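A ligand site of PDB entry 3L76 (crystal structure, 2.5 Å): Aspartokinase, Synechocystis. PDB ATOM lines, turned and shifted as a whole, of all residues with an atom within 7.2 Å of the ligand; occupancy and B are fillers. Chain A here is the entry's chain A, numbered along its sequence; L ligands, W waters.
O of His 540 touches C2 of the ligand, at 3.4 Å.
Pro 541 touches the ligand (CA to O1, 3.9 Å).
Thr 563 touches the ligand.
Glu 565 touches the ligand.
Ile 568 touches the ligand.
Hydrophobic or aromatic side chains that line the ligand: Ile 299, Met 537, Val 543, Ala 544 and Ile 568.
O of Ile 299 sits at hydrogen-bond distance from N1 of the ligand (2.6 Å).
N2 of the ligand sits at hydrogen-bond distance from O of Asp 300 (2.7 Å).
N of Val 543 lies within hydrogen-bond range of O2 of the ligand (3.0 Å).
N of Ile 299 lies within hydrogen-bond range of O1 of the ligand (2.8 Å).
O2 of the ligand sits at hydrogen-bond distance from N of Ala 544 (3.2 Å).
O of Met 537 sits at hydrogen-bond distance from N1 of the ligand (3.0 Å).
The backbone carbonyl oxygen (O) of Ser 564 is in hydrogen-bond range of a nitrogen (N2) of the ligand, at 2.8 Å.
An oxygen (O2) of the ligand lies within hydrogen-bond range of the backbone NH of Gly 542, 3.3 Å away.
N1 of the ligand lies within salt-bridge range of OD1 of Asp 298 (2.8 Å).
Water W2 lies within hydrogen-bond range of O of Val 297, O1 of the ligand and N of Gly 542.
Water W3 lies within hydrogen-bond range of an oxygen (O2) of the ligand, the backbone NH of Ala 545 and the backbone NH of Gly 542.
Water W1 lies within hydrogen-bond range of the backbone carbonyl oxygen (O) of Glu 565 (2.9 Å) and a nitrogen (N2) of the ligand (3.0 Å).
OG1 of Thr 563 sits close to O of Lys 567, at 3.5 Å.
The side-chain hydroxyl (OG) of Ser 564 is in hydrogen-bond range of the backbone NH (N) of Lys 567 (3.3 Å).
OD1 of Asp 298 is in hydrogen-bond range of N of His 540 (2.8 Å).
OG of Ser 564 sits close to N of Ile 566 (3.5 Å).
OD2 of Asp 298 sits close to N of Gly 539 (3.4 Å).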
ATOM      1  N   PHE A 289       1.474  -5.685 -27.176  1.00  0.00           N
ATOM      2  CA  PHE A 289       0.717  -6.880 -27.462  1.00  0.00           C
ATOM      3  C   PHE A 289      -0.083  -6.740 -28.751  1.00  0.00           C
ATOM      4  O   PHE A 289      -0.360  -7.721 -29.426  1.00  0.00           O
ATOM      5  CB  PHE A 289      -0.171  -7.283 -26.262  1.00  0.00           C
ATOM      6  CG  PHE A 289       0.630  -7.668 -25.044  1.00  0.00           C
ATOM      7  CD1 PHE A 289       1.243  -8.909 -24.959  1.00  0.00           C
ATOM      8  CD2 PHE A 289       0.776  -6.783 -23.982  1.00  0.00           C
ATOM      9  CE1 PHE A 289       1.991  -9.268 -23.839  1.00  0.00           C
ATOM     10  CE2 PHE A 289       1.518  -7.130 -22.862  1.00  0.00           C
ATOM     11  CZ  PHE A 289       2.129  -8.370 -22.794  1.00  0.00           C
ATOM     12  N   ILE A 292       2.533  -7.783 -31.367  1.00  0.00           N
ATOM     13  CA  ILE A 292       2.711  -9.234 -31.260  1.00  0.00           C
ATOM     14  C   ILE A 292       1.540 -10.005 -31.867  1.00  0.00           C
ATOM     15  O   ILE A 292       1.732 -11.033 -32.534  1.00  0.00           O
ATOM     16  CB  ILE A 292       2.920  -9.667 -29.816  1.00  0.00           C
ATOM     17  CG1 ILE A 292       4.192  -9.043 -29.254  1.00  0.00           C
ATOM     18  CG2 ILE A 292       2.981 -11.201 -29.714  1.00  0.00           C
ATOM     19  CD1 ILE A 292       4.388  -9.252 -27.761  1.00  0.00           C
ATOM     20  N   ALA A 293       0.321  -9.510 -31.656  1.00  0.00           N
ATOM     21  CA  ALA A 293      -0.856 -10.211 -32.148  1.00  0.00           C
ATOM     22  C   ALA A 293      -0.966 -10.118 -33.656  1.00  0.00           C
ATOM     23  O   ALA A 293      -1.504 -11.015 -34.310  1.00  0.00           O
ATOM     24  CB  ALA A 293      -2.103  -9.677 -31.474  1.00  0.00           C
ATOM     25  N   VAL A 297       0.578 -14.290 -32.943  1.00  0.00           N
ATOM     26  CA  VAL A 297       1.264 -14.993 -31.854  1.00  0.00           C
ATOM     27  C   VAL A 297       0.361 -15.094 -30.629  1.00  0.00           C
ATOM     28  O   VAL A 297       0.079 -14.090 -29.973  1.00  0.00           O
ATOM     29  CB  VAL A 297       2.561 -14.267 -31.455  1.00  0.00           C
ATOM     30  CG1 VAL A 297       3.117 -14.797 -30.131  1.00  0.00           C
ATOM     31  CG2 VAL A 297       3.606 -14.325 -32.572  1.00  0.00           C
ATOM     32  N   ASP A 298      -0.097 -16.302 -30.320  1.00  0.00           N
ATOM     33  CA  ASP A 298      -0.900 -16.495 -29.130  1.00  0.00           C
ATOM     34  C   ASP A 298      -0.048 -16.449 -27.864  1.00  0.00           C
ATOM     35  O   ASP A 298       1.061 -17.002 -27.826  1.00  0.00           O
ATOM     36  CB  ASP A 298      -1.691 -17.806 -29.194  1.00  0.00           C
ATOM     37  CG  ASP A 298      -2.570 -17.996 -27.988  1.00  0.00           C
ATOM     38  OD1 ASP A 298      -3.527 -17.213 -27.813  1.00  0.00           O
ATOM     39  OD2 ASP A 298      -2.299 -18.927 -27.205  1.00  0.00           O
ATOM     40  N   ILE A 299      -0.576 -15.802 -26.835  1.00  0.00           N
ATOM     41  CA  ILE A 299       0.141 -15.668 -25.571  1.00  0.00           C
ATOM     42  C   ILE A 299      -0.543 -16.421 -24.396  1.00  0.00           C
ATOM     43  O   ILE A 299      -1.767 -16.505 -24.318  1.00  0.00           O
ATOM     44  CB  ILE A 299       0.297 -14.180 -25.188  1.00  0.00           C
ATOM     45  CG1 ILE A 299       1.077 -13.443 -26.275  1.00  0.00           C
ATOM     46  CG2 ILE A 299       0.953 -14.024 -23.811  1.00  0.00           C
ATOM     47  CD1 ILE A 299       1.672 -12.156 -25.824  1.00  0.00           C
ATOM     48  N   ASP A 300       0.255 -16.982 -23.500  1.00  0.00           N
ATOM     49  CA  ASP A 300      -0.240 -17.582 -22.261  1.00  0.00           C
ATOM     50  C   ASP A 300      -0.149 -16.641 -21.065  1.00  0.00           C
ATOM     51  O   ASP A 300      -1.055 -15.853 -20.839  1.00  0.00           O
ATOM     52  CB  ASP A 300       0.515 -18.861 -21.938  1.00  0.00           C
ATOM     53  CG  ASP A 300      -0.005 -19.536 -20.670  1.00  0.00           C
ATOM     54  OD1 ASP A 300      -1.183 -19.284 -20.344  1.00  0.00           O
ATOM     55  OD2 ASP A 300       0.734 -20.292 -20.013  1.00  0.00           O
ATOM     56  N   LEU A 301       0.933 -16.730 -20.287  1.00  0.00           N
ATOM     57  CA  LEU A 301       1.139 -15.868 -19.134  1.00  0.00           C
ATOM     58  C   LEU A 301       1.441 -14.409 -19.521  1.00  0.00           C
ATOM     59  O   LEU A 301       2.249 -14.132 -20.416  1.00  0.00           O
ATOM     60  CB  LEU A 301       2.270 -16.389 -18.248  1.00  0.00           C
ATOM     61  CG  LEU A 301       1.999 -17.568 -17.300  1.00  0.00           C
ATOM     62  CD1 LEU A 301       3.310 -18.192 -16.861  1.00  0.00           C
ATOM     63  CD2 LEU A 301       1.171 -17.130 -16.086  1.00  0.00           C
ATOM     64  N   ILE A 302       0.797 -13.475 -18.838  1.00  0.00           N
ATOM     65  CA  ILE A 302       1.228 -12.089 -18.839  1.00  0.00           C
ATOM     66  C   ILE A 302       1.380 -11.627 -17.395  1.00  0.00           C
ATOM     67  O   ILE A 302       0.416 -11.621 -16.608  1.00  0.00           O
ATOM     68  CB  ILE A 302       0.262 -11.167 -19.610  1.00  0.00           C
ATOM     69  CG1 ILE A 302       0.042 -11.692 -21.031  1.00  0.00           C
ATOM     70  CG2 ILE A 302       0.796  -9.719 -19.643  1.00  0.00           C
ATOM     71  CD1 ILE A 302      -0.880 -10.825 -21.859  1.00  0.00           C
ATOM     72  N   GLY A 536     -12.714 -18.663 -24.495  1.00  0.00           N
ATOM     73  CA  GLY A 536     -12.320 -18.505 -25.880  1.00  0.00           C
ATOM     74  C   GLY A 536     -10.980 -17.829 -26.097  1.00  0.00           C
ATOM     75  O   GLY A 536     -10.480 -17.804 -27.219  1.00  0.00           O
ATOM     76  N   MET A 537     -10.377 -17.290 -25.048  1.00  0.00           N
ATOM     77  CA  MET A 537      -9.132 -16.534 -25.231  1.00  0.00           C
ATOM     78  C   MET A 537      -7.923 -17.461 -25.390  1.00  0.00           C
ATOM     79  O   MET A 537      -6.845 -17.027 -25.771  1.00  0.00           O
ATOM     80  CB  MET A 537      -8.936 -15.488 -24.133  1.00  0.00           C
ATOM     81  CG  MET A 537      -8.412 -15.994 -22.799  1.00  0.00           C
ATOM     82  SD  MET A 537      -8.068 -14.661 -21.628  1.00  0.00           S
ATOM     83  CE  MET A 537      -9.625 -13.791 -21.614  1.00  0.00           C
ATOM     84  N   ILE A 538      -8.130 -18.748 -25.124  1.00  0.00           N
ATOM     85  CA  ILE A 538      -7.088 -19.749 -25.288  1.00  0.00           C
ATOM     86  C   ILE A 538      -6.788 -20.032 -26.767  1.00  0.00           C
ATOM     87  O   ILE A 538      -7.691 -20.352 -27.548  1.00  0.00           O
ATOM     88  CB  ILE A 538      -7.478 -21.065 -24.595  1.00  0.00           C
ATOM     89  CG1 ILE A 538      -7.666 -20.841 -23.095  1.00  0.00           C
ATOM     90  CG2 ILE A 538      -6.437 -22.125 -24.833  1.00  0.00           C
ATOM     91  CD1 ILE A 538      -8.145 -22.097 -22.356  1.00  0.00           C
ATOM     92  N   GLY A 539      -5.527 -19.897 -27.154  1.00  0.00           N
ATOM     93  CA  GLY A 539      -5.154 -20.074 -28.540  1.00  0.00           C
ATOM     94  C   GLY A 539      -5.818 -19.050 -29.441  1.00  0.00           C
ATOM     95  O   GLY A 539      -6.179 -19.362 -30.574  1.00  0.00           O
ATOM     96  N   HIS A 540      -5.976 -17.838 -28.934  1.00  0.00           N
ATOM     97  CA  HIS A 540      -6.655 -16.757 -29.660  1.00  0.00           C
ATOM     98  C   HIS A 540      -5.861 -15.456 -29.509  1.00  0.00           C
ATOM     99  O   HIS A 540      -6.029 -14.715 -28.542  1.00  0.00           O
ATOM    100  CB  HIS A 540      -8.079 -16.608 -29.105  1.00  0.00           C
ATOM    101  CG  HIS A 540      -8.957 -15.721 -29.940  1.00  0.00           C
ATOM    102  ND1 HIS A 540      -8.993 -14.357 -29.773  1.00  0.00           N
ATOM    103  CD2 HIS A 540      -9.833 -16.005 -30.929  1.00  0.00           C
ATOM    104  CE1 HIS A 540      -9.854 -13.833 -30.630  1.00  0.00           C
ATOM    105  NE2 HIS A 540     -10.380 -14.816 -31.342  1.00  0.00           N
ATOM    106  N   PRO A 541      -4.974 -15.164 -30.467  1.00  0.00           N
ATOM    107  CA  PRO A 541      -4.115 -13.980 -30.323  1.00  0.00           C
ATOM    108  C   PRO A 541      -4.901 -12.681 -30.299  1.00  0.00           C
ATOM    109  O   PRO A 541      -5.974 -12.588 -30.903  1.00  0.00           O
ATOM    110  CB  PRO A 541      -3.209 -14.056 -31.555  1.00  0.00           C
ATOM    111  CG  PRO A 541      -3.194 -15.500 -31.928  1.00  0.00           C
ATOM    112  CD  PRO A 541      -4.573 -16.012 -31.598  1.00  0.00           C
ATOM    113  N   GLY A 542      -4.387 -11.689 -29.580  1.00  0.00           N
ATOM    114  CA  GLY A 542      -4.971 -10.362 -29.566  1.00  0.00           C
ATOM    115  C   GLY A 542      -6.054 -10.078 -28.542  1.00  0.00           C
ATOM    116  O   GLY A 542      -6.584  -8.966 -28.548  1.00  0.00           O
ATOM    117  N   VAL A 543      -6.377 -11.037 -27.673  1.00  0.00           N
ATOM    118  CA  VAL A 543      -7.381 -10.765 -26.636  1.00  0.00           C
ATOM    119  C   VAL A 543      -6.834  -9.809 -25.577  1.00  0.00           C
ATOM    120  O   VAL A 543      -7.423  -8.774 -25.265  1.00  0.00           O
ATOM    121  CB  VAL A 543      -7.890 -12.040 -25.951  1.00  0.00           C
ATOM    122  CG1 VAL A 543      -8.780 -11.676 -24.774  1.00  0.00           C
ATOM    123  CG2 VAL A 543      -8.648 -12.907 -26.938  1.00  0.00           C
ATOM    124  N   ALA A 544      -5.698 -10.160 -25.005  1.00  0.00           N
ATOM    125  CA  ALA A 544      -5.084  -9.256 -24.052  1.00  0.00           C
ATOM    126  C   ALA A 544      -4.819  -7.881 -24.707  1.00  0.00           C
ATOM    127  O   ALA A 544      -5.000  -6.847 -24.070  1.00  0.00           O
ATOM    128  CB  ALA A 544      -3.802  -9.858 -23.529  1.00  0.00           C
ATOM    129  N   ALA A 545      -4.419  -7.888 -25.972  1.00  0.00           N
ATOM    130  CA  ALA A 545      -4.090  -6.639 -26.638  1.00  0.00           C
ATOM    131  C   ALA A 545      -5.319  -5.743 -26.720  1.00  0.00           C
ATOM    132  O   ALA A 545      -5.240  -4.539 -26.472  1.00  0.00           O
ATOM    133  CB  ALA A 545      -3.508  -6.885 -28.015  1.00  0.00           C
ATOM    134  N   HIS A 546      -6.458  -6.331 -27.062  1.00  0.00           N
ATOM    135  CA  HIS A 546      -7.687  -5.567 -27.147  1.00  0.00           C
ATOM    136  C   HIS A 546      -8.078  -4.955 -25.809  1.00  0.00           C
ATOM    137  O   HIS A 546      -8.503  -3.815 -25.743  1.00  0.00           O
ATOM    138  CB  HIS A 546      -8.827  -6.436 -27.651  1.00  0.00           C
ATOM    139  CG  HIS A 546      -9.954  -5.655 -28.234  1.00  0.00           C
ATOM    140  ND1 HIS A 546      -9.765  -4.652 -29.168  1.00  0.00           N
ATOM    141  CD2 HIS A 546     -11.297  -5.727 -28.030  1.00  0.00           C
ATOM    142  CE1 HIS A 546     -10.932  -4.145 -29.506  1.00  0.00           C
ATOM    143  NE2 HIS A 546     -11.884  -4.773 -28.829  1.00  0.00           N
ATOM    144  N   PHE A 548      -6.026  -4.216 -23.164  1.00  0.00           N
ATOM    145  CA  PHE A 548      -5.109  -3.130 -22.833  1.00  0.00           C
ATOM    146  C   PHE A 548      -5.337  -1.882 -23.704  1.00  0.00           C
ATOM    147  O   PHE A 548      -5.200  -0.754 -23.229  1.00  0.00           O
ATOM    148  CB  PHE A 548      -3.657  -3.584 -22.988  1.00  0.00           C
ATOM    149  CG  PHE A 548      -3.337  -4.833 -22.234  1.00  0.00           C
ATOM    150  CD1 PHE A 548      -4.025  -5.146 -21.063  1.00  0.00           C
ATOM    151  CD2 PHE A 548      -2.351  -5.686 -22.679  1.00  0.00           C
ATOM    152  CE1 PHE A 548      -3.731  -6.312 -20.354  1.00  0.00           C
ATOM    153  CE2 PHE A 548      -2.036  -6.850 -21.979  1.00  0.00           C
ATOM    154  CZ  PHE A 548      -2.731  -7.150 -20.807  1.00  0.00           C
ATOM    155  N   ALA A 562      -1.974  -9.530 -14.249  1.00  0.00           N
ATOM    156  CA  ALA A 562      -1.873 -10.934 -13.841  1.00  0.00           C
ATOM    157  C   ALA A 562      -2.862 -11.819 -14.604  1.00  0.00           C
ATOM    158  O   ALA A 562      -3.948 -11.391 -14.974  1.00  0.00           O
ATOM    159  CB  ALA A 562      -2.058 -11.104 -12.332  1.00  0.00           C
ATOM    160  N   THR A 563      -2.488 -13.062 -14.812  1.00  0.00           N
ATOM    161  CA  THR A 563      -3.189 -13.849 -15.808  1.00  0.00           C
ATOM    162  C   THR A 563      -3.436 -15.307 -15.382  1.00  0.00           C
ATOM    163  O   THR A 563      -2.752 -15.833 -14.506  1.00  0.00           O
ATOM    164  CB  THR A 563      -2.400 -13.757 -17.134  1.00  0.00           C
ATOM    165  OG1 THR A 563      -3.224 -13.210 -18.166  1.00  0.00           O
ATOM    166  CG2 THR A 563      -1.821 -15.064 -17.526  1.00  0.00           C
ATOM    167  N   SER A 564      -4.470 -15.910 -15.952  1.00  0.00           N
ATOM    168  CA  SER A 564      -4.525 -17.379 -16.082  1.00  0.00           C
ATOM    169  C   SER A 564      -4.860 -17.652 -17.540  1.00  0.00           C
ATOM    170  O   SER A 564      -4.900 -16.732 -18.353  1.00  0.00           O
ATOM    171  CB  SER A 564      -5.541 -18.007 -15.128  1.00  0.00           C
ATOM    172  OG  SER A 564      -6.869 -17.741 -15.515  1.00  0.00           O
ATOM    173  N   GLU A 565      -5.090 -18.902 -17.912  1.00  0.00           N
ATOM    174  CA  GLU A 565      -5.411 -19.179 -19.314  1.00  0.00           C
ATOM    175  C   GLU A 565      -6.692 -18.485 -19.793  1.00  0.00           C
ATOM    176  O   GLU A 565      -6.861 -18.260 -20.987  1.00  0.00           O
ATOM    177  CB  GLU A 565      -5.517 -20.680 -19.581  1.00  0.00           C
ATOM    178  CG  GLU A 565      -4.300 -21.501 -19.167  1.00  0.00           C
ATOM    179  CD  GLU A 565      -4.258 -21.740 -17.675  1.00  0.00           C
ATOM    180  OE1 GLU A 565      -5.223 -21.344 -16.984  1.00  0.00           O
ATOM    181  OE2 GLU A 565      -3.269 -22.331 -17.212  1.00  0.00           O
ATOM    182  N   ILE A 566      -7.598 -18.149 -18.881  1.00  0.00           N
ATOM    183  CA  ILE A 566      -8.899 -17.598 -19.284  1.00  0.00           C
ATOM    184  C   ILE A 566      -9.307 -16.337 -18.541  1.00  0.00           C
ATOM    185  O   ILE A 566     -10.397 -15.816 -18.739  1.00  0.00           O
ATOM    186  CB  ILE A 566     -10.037 -18.676 -19.178  1.00  0.00           C
ATOM    187  CG1 ILE A 566     -10.431 -18.930 -17.722  1.00  0.00           C
ATOM    188  CG2 ILE A 566      -9.638 -19.983 -19.849  1.00  0.00           C
ATOM    189  CD1 ILE A 566     -11.557 -19.941 -17.572  1.00  0.00           C
ATOM    190  N   LYS A 567      -8.418 -15.832 -17.687  1.00  0.00           N
ATOM    191  CA  LYS A 567      -8.673 -14.595 -16.952  1.00  0.00           C
ATOM    192  C   LYS A 567      -7.493 -13.645 -17.078  1.00  0.00           C
ATOM    193  O   LYS A 567      -6.352 -14.043 -16.861  1.00  0.00           O
ATOM    194  CB  LYS A 567      -8.928 -14.857 -15.467  1.00  0.00           C
ATOM    195  CG  LYS A 567      -9.379 -13.615 -14.700  1.00  0.00           C
ATOM    196  CD  LYS A 567      -9.728 -13.934 -13.230  1.00  0.00           C
ATOM    197  CE  LYS A 567     -10.680 -12.879 -12.643  1.00  0.00           C
ATOM    198  NZ  LYS A 567     -10.675 -12.909 -11.163  1.00  0.00           N
ATOM    199  N   ILE A 568      -7.780 -12.403 -17.463  1.00  0.00           N
ATOM    200  CA  ILE A 568      -6.803 -11.319 -17.385  1.00  0.00           C
ATOM    201  C   ILE A 568      -7.302 -10.278 -16.392  1.00  0.00           C
ATOM    202  O   ILE A 568      -8.435  -9.819 -16.483  1.00  0.00           O
ATOM    203  CB  ILE A 568      -6.539 -10.639 -18.752  1.00  0.00           C
ATOM    204  CG1 ILE A 568      -6.111 -11.663 -19.806  1.00  0.00           C
ATOM    205  CG2 ILE A 568      -5.443  -9.597 -18.607  1.00  0.00           C
ATOM    206  CD1 ILE A 568      -6.461 -11.247 -21.219  1.00  0.00           C
HETATM  207  N1  LIG L   1      -4.065 -15.996 -25.344  1.00  0.00           N
HETATM  208  C1  LIG L   1      -4.647 -14.661 -25.325  1.00  0.00           C
HETATM  209  C2  LIG L   1      -3.791 -13.713 -26.166  1.00  0.00           C
HETATM  210  O1  LIG L   1      -2.730 -14.096 -26.684  1.00  0.00           O
HETATM  211  C3  LIG L   1      -4.813 -14.146 -23.887  1.00  0.00           C
HETATM  212  C4  LIG L   1      -3.517 -14.142 -23.035  1.00  0.00           C
HETATM  213  C5  LIG L   1      -3.791 -13.605 -21.618  1.00  0.00           C
HETATM  214  C6  LIG L   1      -4.487 -14.645 -20.738  1.00  0.00           C
HETATM  215  N2  LIG L   1      -3.708 -15.934 -20.721  1.00  0.00           N
HETATM  216  O2  LIG L   1      -4.149 -12.547 -26.377  1.00  0.00           O
HETATM  217  O   HOH W   1      -4.730 -17.782 -22.827  1.00  0.00           O
HETATM  218  O   HOH W   2      -1.593 -12.576 -28.676  1.00  0.00           O
HETATM  219  O   HOH W   3      -2.913 -10.053 -27.355  1.00  0.00           O
